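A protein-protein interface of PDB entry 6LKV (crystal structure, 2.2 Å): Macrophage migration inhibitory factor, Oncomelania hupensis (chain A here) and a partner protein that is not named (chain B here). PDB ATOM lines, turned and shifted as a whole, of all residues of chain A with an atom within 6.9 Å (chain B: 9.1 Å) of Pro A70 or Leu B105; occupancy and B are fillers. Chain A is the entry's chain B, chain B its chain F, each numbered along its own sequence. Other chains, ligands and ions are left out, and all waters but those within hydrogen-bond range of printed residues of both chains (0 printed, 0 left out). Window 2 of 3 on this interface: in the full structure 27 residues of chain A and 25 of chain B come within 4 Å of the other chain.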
ATOM      1  N   LEU A  68      16.434   7.478  15.633  1.00  0.00           N
ATOM      2  CA  LEU A  68      17.726   8.073  15.221  1.00  0.00           C
ATOM      3  C   LEU A  68      18.506   7.080  14.361  1.00  0.00           C
ATOM      4  O   LEU A  68      18.787   5.958  14.845  1.00  0.00           O
ATOM      5  CB  LEU A  68      18.518   8.498  16.471  1.00  0.00           C
ATOM      6  CG  LEU A  68      17.744   9.364  17.481  1.00  0.00           C
ATOM      7  CD1 LEU A  68      18.641   9.758  18.649  1.00  0.00           C
ATOM      8  CD2 LEU A  68      17.167  10.610  16.813  1.00  0.00           C
ATOM      9  N   ASN A  69      18.922   7.529  13.166  1.00  0.00           N
ATOM     10  CA  ASN A  69      19.750   6.769  12.199  1.00  0.00           C
ATOM     11  C   ASN A  69      20.414   7.787  11.282  1.00  0.00           C
ATOM     12  O   ASN A  69      19.995   8.945  11.236  1.00  0.00           O
ATOM     13  CB  ASN A  69      18.895   5.741  11.450  1.00  0.00           C
ATOM     14  CG  ASN A  69      17.795   6.392  10.630  1.00  0.00           C
ATOM     15  OD1 ASN A  69      18.086   7.098   9.665  1.00  0.00           O
ATOM     16  ND2 ASN A  69      16.556   6.232  11.063  1.00  0.00           N
ATOM     17  N   PRO A  70      21.453   7.408  10.512  1.00  0.00           N
ATOM     18  CA  PRO A  70      22.175   8.377   9.697  1.00  0.00           C
ATOM     19  C   PRO A  70      21.256   9.229   8.805  1.00  0.00           C
ATOM     20  O   PRO A  70      21.526  10.421   8.638  1.00  0.00           O
ATOM     21  CB  PRO A  70      23.135   7.505   8.881  1.00  0.00           C
ATOM     22  CG  PRO A  70      23.373   6.304   9.773  1.00  0.00           C
ATOM     23  CD  PRO A  70      22.029   6.060  10.429  1.00  0.00           C
ATOM     24  N   THR A  71      20.186   8.641   8.270  1.00  0.00           N
ATOM     25  CA  THR A  71      19.281   9.325   7.309  1.00  0.00           C
ATOM     26  C   THR A  71      18.421  10.337   8.059  1.00  0.00           C
ATOM     27  O   THR A  71      18.396  11.499   7.635  1.00  0.00           O
ATOM     28  CB  THR A  71      18.476   8.310   6.476  1.00  0.00           C
ATOM     29  OG1 THR A  71      19.439   7.717   5.592  1.00  0.00           O
ATOM     30  CG2 THR A  71      17.358   8.921   5.666  1.00  0.00           C
ATOM     31  N   SER A  72      17.693   9.906   9.091  1.00  0.00           N
ATOM     32  CA  SER A  72      16.805  10.798   9.890  1.00  0.00           C
ATOM     33  C   SER A  72      17.665  11.894  10.570  1.00  0.00           C
ATOM     34  O   SER A  72      17.262  13.046  10.573  1.00  0.00           O
ATOM     35  CB  SER A  72      15.966  10.018  10.857  1.00  0.00           C
ATOM     36  OG  SER A  72      16.768   9.399  11.861  1.00  0.00           O
ATOM     37  N   ASN A  73      18.874  11.570  11.014  1.00  0.00           N
ATOM     38  CA  ASN A  73      19.762  12.501  11.753  1.00  0.00           C
ATOM     39  C   ASN A  73      20.110  13.688  10.850  1.00  0.00           C
ATOM     40  O   ASN A  73      19.963  14.842  11.312  1.00  0.00           O
ATOM     41  CB  ASN A  73      21.031  11.814  12.257  1.00  0.00           C
ATOM     42  CG  ASN A  73      20.754  10.828  13.378  1.00  0.00           C
ATOM     43  OD1 ASN A  73      19.650  10.751  13.917  1.00  0.00           O
ATOM     44  ND2 ASN A  73      21.753  10.036  13.705  1.00  0.00           N
ATOM     45  N   LEU A  74      20.541  13.424   9.607  1.00  0.00           N
ATOM     46  CA  LEU A  74      20.913  14.494   8.653  1.00  0.00           C
ATOM     47  C   LEU A  74      19.690  15.386   8.374  1.00  0.00           C
ATOM     48  O   LEU A  74      19.831  16.634   8.419  1.00  0.00           O
ATOM     49  CB  LEU A  74      21.472  13.893   7.360  1.00  0.00           C
ATOM     50  CG  LEU A  74      21.833  14.917   6.280  1.00  0.00           C
ATOM     51  CD1 LEU A  74      22.846  15.924   6.790  1.00  0.00           C
ATOM     52  CD2 LEU A  74      22.349  14.232   5.014  1.00  0.00           C
ATOM     53  N   ALA A  75      18.535  14.784   8.109  1.00  0.00           N
ATOM     54  CA  ALA A  75      17.311  15.535   7.771  1.00  0.00           C
ATOM     55  C   ALA A  75      16.918  16.418   8.959  1.00  0.00           C
ATOM     56  O   ALA A  75      16.607  17.594   8.745  1.00  0.00           O
ATOM     57  CB  ALA A  75      16.186  14.602   7.373  1.00  0.00           C
ATOM     58  N   PHE A  99      22.917  13.609  18.301  1.00  0.00           N
ATOM     59  CA  PHE A  99      21.749  12.699  18.334  1.00  0.00           C
ATOM     60  C   PHE A  99      22.147  11.547  19.258  1.00  0.00           C
ATOM     61  O   PHE A  99      23.194  10.925  19.020  1.00  0.00           O
ATOM     62  CB  PHE A  99      21.371  12.276  16.905  1.00  0.00           C
ATOM     63  CG  PHE A  99      20.984  13.435  16.026  1.00  0.00           C
ATOM     64  CD1 PHE A  99      19.676  13.870  16.002  1.00  0.00           C
ATOM     65  CD2 PHE A  99      21.919  14.102  15.251  1.00  0.00           C
ATOM     66  CE1 PHE A  99      19.310  14.964  15.239  1.00  0.00           C
ATOM     67  CE2 PHE A  99      21.546  15.205  14.490  1.00  0.00           C
ATOM     68  CZ  PHE A  99      20.247  15.623  14.476  1.00  0.00           C
ATOM     69  N   ILE B  65      34.076  12.939  18.520  1.00  0.00           N
ATOM     70  CA  ILE B  65      34.052  11.859  17.492  1.00  0.00           C
ATOM     71  C   ILE B  65      35.487  11.355  17.356  1.00  0.00           C
ATOM     72  O   ILE B  65      36.365  12.167  17.053  1.00  0.00           O
ATOM     73  CB  ILE B  65      33.484  12.354  16.156  1.00  0.00           C
ATOM     74  CG1 ILE B  65      32.089  12.949  16.344  1.00  0.00           C
ATOM     75  CG2 ILE B  65      33.462  11.218  15.141  1.00  0.00           C
ATOM     76  CD1 ILE B  65      31.639  13.817  15.198  1.00  0.00           C
ATOM     77  N   VAL B 102      31.180   9.998  20.515  1.00  0.00           N
ATOM     78  CA  VAL B 102      30.039  10.445  19.671  1.00  0.00           C
ATOM     79  C   VAL B 102      30.186   9.770  18.300  1.00  0.00           C
ATOM     80  O   VAL B 102      31.256   9.829  17.696  1.00  0.00           O
ATOM     81  CB  VAL B 102      30.031  11.983  19.540  1.00  0.00           C
ATOM     82  CG1 VAL B 102      28.913  12.469  18.636  1.00  0.00           C
ATOM     83  CG2 VAL B 102      29.957  12.649  20.902  1.00  0.00           C
ATOM     84  N   PRO B 103      29.158   9.055  17.796  1.00  0.00           N
ATOM     85  CA  PRO B 103      29.214   8.494  16.435  1.00  0.00           C
ATOM     86  C   PRO B 103      29.162   9.602  15.377  1.00  0.00           C
ATOM     87  O   PRO B 103      28.392  10.544  15.520  1.00  0.00           O
ATOM     88  CB  PRO B 103      27.960   7.615  16.326  1.00  0.00           C
ATOM     89  CG  PRO B 103      27.462   7.449  17.763  1.00  0.00           C
ATOM     90  CD  PRO B 103      27.911   8.704  18.496  1.00  0.00           C
ATOM     91  N   ALA B 104      29.979   9.462  14.339  1.00  0.00           N
ATOM     92  CA  ALA B 104      30.144  10.417  13.216  1.00  0.00           C
ATOM     93  C   ALA B 104      28.804  10.721  12.546  1.00  0.00           C
ATOM     94  O   ALA B 104      28.581  11.863  12.156  1.00  0.00           O
ATOM     95  CB  ALA B 104      31.127   9.874  12.207  1.00  0.00           C
ATOM     96  N   LEU B 105      27.938   9.737  12.430  1.00  0.00           N
ATOM     97  CA  LEU B 105      26.651   9.847  11.719  1.00  0.00           C
ATOM     98  C   LEU B 105      25.538  10.231  12.703  1.00  0.00           C
ATOM     99  O   LEU B 105      24.387  10.270  12.270  1.00  0.00           O
ATOM    100  CB  LEU B 105      26.375   8.506  11.021  1.00  0.00           C
ATOM    101  CG  LEU B 105      27.418   8.067   9.988  1.00  0.00           C
ATOM    102  CD1 LEU B 105      27.033   6.720   9.381  1.00  0.00           C
ATOM    103  CD2 LEU B 105      27.592   9.129   8.905  1.00  0.00           C
ATOM    104  N   PHE B 106      25.884  10.534  13.963  1.00  0.00           N
ATOM    105  CA  PHE B 106      24.926  10.952  15.023  1.00  0.00           C
ATOM    106  C   PHE B 106      25.324  12.355  15.510  1.00  0.00           C
ATOM    107  O   PHE B 106      25.028  12.737  16.662  1.00  0.00           O
ATOM    108  CB  PHE B 106      24.879   9.896  16.132  1.00  0.00           C
ATOM    109  CG  PHE B 106      24.065   8.681  15.786  1.00  0.00           C
ATOM    110  CD1 PHE B 106      24.503   7.783  14.811  1.00  0.00           C
ATOM    111  CD2 PHE B 106      22.868   8.417  16.424  1.00  0.00           C
ATOM    112  CE1 PHE B 106      23.748   6.657  14.488  1.00  0.00           C
ATOM    113  CE2 PHE B 106      22.114   7.296  16.094  1.00  0.00           C
ATOM    114  CZ  PHE B 106      22.546   6.426  15.105  1.00  0.00           C
ATOM    115  N   CYS B 107      25.992  13.116  14.646  1.00  0.00           N
ATOM    116  CA  CYS B 107      26.473  14.475  14.948  1.00  0.00           C
ATOM    117  C   CYS B 107      26.615  15.290  13.658  1.00  0.00           C
ATOM    118  O   CYS B 107      27.422  14.896  12.768  1.00  0.00           O
ATOM    119  CB  CYS B 107      27.794  14.425  15.702  1.00  0.00           C
ATOM    120  SG  CYS B 107      28.314  16.046  16.313  1.00  0.00           S
ATOM    121  N   SER B 108      25.902  16.413  13.585  1.00  0.00           N
ATOM    122  CA  SER B 108      25.953  17.411  12.487  1.00  0.00           C
ATOM    123  C   SER B 108      26.867  18.589  12.841  1.00  0.00           C
ATOM    124  O   SER B 108      26.956  18.990  14.035  1.00  0.00           O
ATOM    125  CB  SER B 108      24.598  17.887  12.135  1.00  0.00           C
ATOM    126  OG  SER B 108      23.938  18.491  13.253  1.00  0.00           O
ATOM    127  N   ALA B 112      25.947  19.139   7.532  1.00  0.00           N
ATOM    128  CA  ALA B 112      26.348  17.756   7.170  1.00  0.00           C
ATOM    129  C   ALA B 112      26.726  16.935   8.409  1.00  0.00           C
ATOM    130  O   ALA B 112      27.102  17.543   9.448  1.00  0.00           O
ATOM    131  CB  ALA B 112      27.506  17.822   6.204  1.00  0.00           C
ATOM    132  N   LEU B 113      26.703  15.603   8.265  1.00  0.00           N
ATOM    133  CA  LEU B 113      27.212  14.693   9.315  1.00  0.00           C
ATOM    134  C   LEU B 113      28.727  14.670   9.215  1.00  0.00           C
ATOM    135  O   LEU B 113      29.306  15.538   8.504  1.00  0.00           O
ATOM    136  CB  LEU B 113      26.594  13.310   9.177  1.00  0.00           C
ATOM    137  CG  LEU B 113      25.071  13.267   9.128  1.00  0.00           C
ATOM    138  CD1 LEU B 113      24.575  11.841   9.038  1.00  0.00           C
ATOM    139  CD2 LEU B 113      24.439  13.953  10.336  1.00  0.00           C
ATOM    140  N   HIS B 114      29.367  13.769   9.948  1.00  0.00           N
ATOM    141  CA  HIS B 114      30.846  13.622   9.953  1.00  0.00           C
ATOM    142  C   HIS B 114      31.212  12.316   9.254  1.00  0.00           C
ATOM    143  O   HIS B 114      30.352  11.414   9.180  1.00  0.00           O
ATOM    144  CB  HIS B 114      31.369  13.709  11.388  1.00  0.00           C
ATOM    145  CG  HIS B 114      31.209  15.053  12.016  1.00  0.00           C
ATOM    146  ND1 HIS B 114      29.988  15.517  12.489  1.00  0.00           N
ATOM    147  CD2 HIS B 114      32.112  16.026  12.272  1.00  0.00           C
ATOM    148  CE1 HIS B 114      30.163  16.715  13.014  1.00  0.00           C
ATOM    149  NE2 HIS B 114      31.448  17.057  12.891  1.00  0.00           N
ATOM    150  N   ASP B 115      32.454  12.197   8.795  1.00  0.00           N
ATOM    151  CA  ASP B 115      32.856  11.221   7.744  1.00  0.00           C
ATOM    152  C   ASP B 115      32.506   9.774   8.155  1.00  0.00           C
ATOM    153  O   ASP B 115      31.622   9.176   7.506  1.00  0.00           O
ATOM    154  CB  ASP B 115      34.310  11.423   7.379  1.00  0.00           C
ATOM    155  N   VAL B 116      33.114   9.276   9.229  1.00  0.00           N
ATOM    156  CA  VAL B 116      32.836   7.981   9.923  1.00  0.00           C
ATOM    157  C   VAL B 116      34.191   7.294  10.123  1.00  0.00           C
ATOM    158  O   VAL B 116      34.407   6.673  11.198  1.00  0.00           O
ATOM    159  CB  VAL B 116      31.813   7.039   9.262  1.00  0.00           C
ATOM    160  CG1 VAL B 116      32.282   6.547   7.903  1.00  0.00           C
ATOM    161  CG2 VAL B 116      31.485   5.850  10.161  1.00  0.00           C
ATOM    162  N   SER B 117      35.124   7.645   9.253  1.00  0.00           N
ATOM    163  CA  SER B 117      36.524   7.194   9.374  1.00  0.00           C
ATOM    164  C   SER B 117      37.120   7.879  10.603  1.00  0.00           C
ATOM    165  O   SER B 117      38.034   7.320  11.196  1.00  0.00           O
ATOM    166  CB  SER B 117      37.274   7.568   8.142  1.00  0.00           C
ATOM    167  OG  SER B 117      36.903   8.864   7.731  1.00  0.00           O
ATOM    168  N   ILE B 118      36.585   9.049  10.958  1.00  0.00           N
ATOM    169  CA  ILE B 118      37.063   9.865  12.115  1.00  0.00           C
ATOM    170  C   ILE B 118      36.839   9.069  13.402  1.00  0.00           C
ATOM    171  O   ILE B 118      37.709   9.161  14.293  1.00  0.00           O
ATOM    172  CB  ILE B 118      36.364  11.236  12.186  1.00  0.00           C
ATOM    173  CG1 ILE B 118      36.424  12.019  10.865  1.00  0.00           C
ATOM    174  CG2 ILE B 118      36.899  12.016  13.386  1.00  0.00           C
ATOM    175  CD1 ILE B 118      37.582  13.012  10.700  1.00  0.00           C
ATOM    176  N   GLU B 119      35.767   8.268  13.488  1.00  0.00           N
ATOM    177  CA  GLU B 119      35.440   7.519  14.726  1.00  0.00           C
ATOM    178  C   GLU B 119      36.604   6.626  15.133  1.00  0.00           C
ATOM    179  O   GLU B 119      36.778   6.387  16.356  1.00  0.00           O
ATOM    180  CB  GLU B 119      34.279   6.559  14.543  1.00  0.00           C
ATOM    181  CG  GLU B 119      32.945   7.219  14.572  1.00  0.00           C
ATOM    182  CD  GLU B 119      31.822   6.262  14.261  1.00  0.00           C
ATOM    183  OE1 GLU B 119      32.102   5.057  14.133  1.00  0.00           O
ATOM    184  OE2 GLU B 119      30.696   6.734  14.069  1.00  0.00           O
ATOM    185  N   ARG B 120      37.307   6.079  14.138  1.00  0.00           N
ATOM    186  CA  ARG B 120      38.411   5.110  14.357  1.00  0.00           C
ATOM    187  C   ARG B 120      39.748   5.836  14.184  1.00  0.00           C
ATOM    188  O   ARG B 120      40.760   5.158  14.107  1.00  0.00           O
ATOM    189  CB  ARG B 120      38.261   3.906  13.415  1.00  0.00           C
ATOM    190  CG  ARG B 120      37.041   3.027  13.679  1.00  0.00           C
ATOM    191  CD  ARG B 120      36.908   1.862  12.703  1.00  0.00           C
ATOM    192  NE  ARG B 120      36.869   2.290  11.302  1.00  0.00           N
ATOM    193  CZ  ARG B 120      35.806   2.797  10.666  1.00  0.00           C
ATOM    194  NH1 ARG B 120      34.652   2.935  11.295  1.00  0.00           N
ATOM    195  NH2 ARG B 120      35.897   3.149   9.391  1.00  0.00           N
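The backbone carbonyl oxygen (O) of Phe B106 is in hydrogen-bond range of the backbone NH (N) of Phe A99, at 2.8 Å.
ND2 of Asn A73 lies within hydrogen-bond range of O of Leu B105.
The side-chain amide nitrogen (ND2) of Asn A73 lies close to the backbone carbonyl oxygen (O) of Asn A69, at 3.2 Å.
Among the printed residues, merely in contact across the chains: Asn A73 with Phe B106 (3.4 Å), Pro A70 with Leu B113 (3.4 Å), Pro A70 with Leu B105 (3.7 Å), Leu A68 with Phe B106 (3.8 Å), Leu A74 with Leu B113 (3.9 Å) and Leu A74 with Ala B112 (3.97 Å).
Pro A70 touches two residues of chain B.
Leu B105 touches just these residues of chain A: Pro A70 and Asn A73.
Of the printed residues of chain A, Leu B113 touches Pro A70 and Leu A74.
Printed residues of chain B within 4 Å of Leu A68: Phe B106 (3.8 Å).
The nearest residue of chain B that does not touch Pro A70 is Phe B106 (4.4 Å).
Of the 9 printed residues of chain A, 5 touch a printed residue of chain B.
Hydrophobic or aromatic side chains of chain A within 4 Å of the printed part of chain B: Leu A68, Pro A70, Leu A74 and Phe A99.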
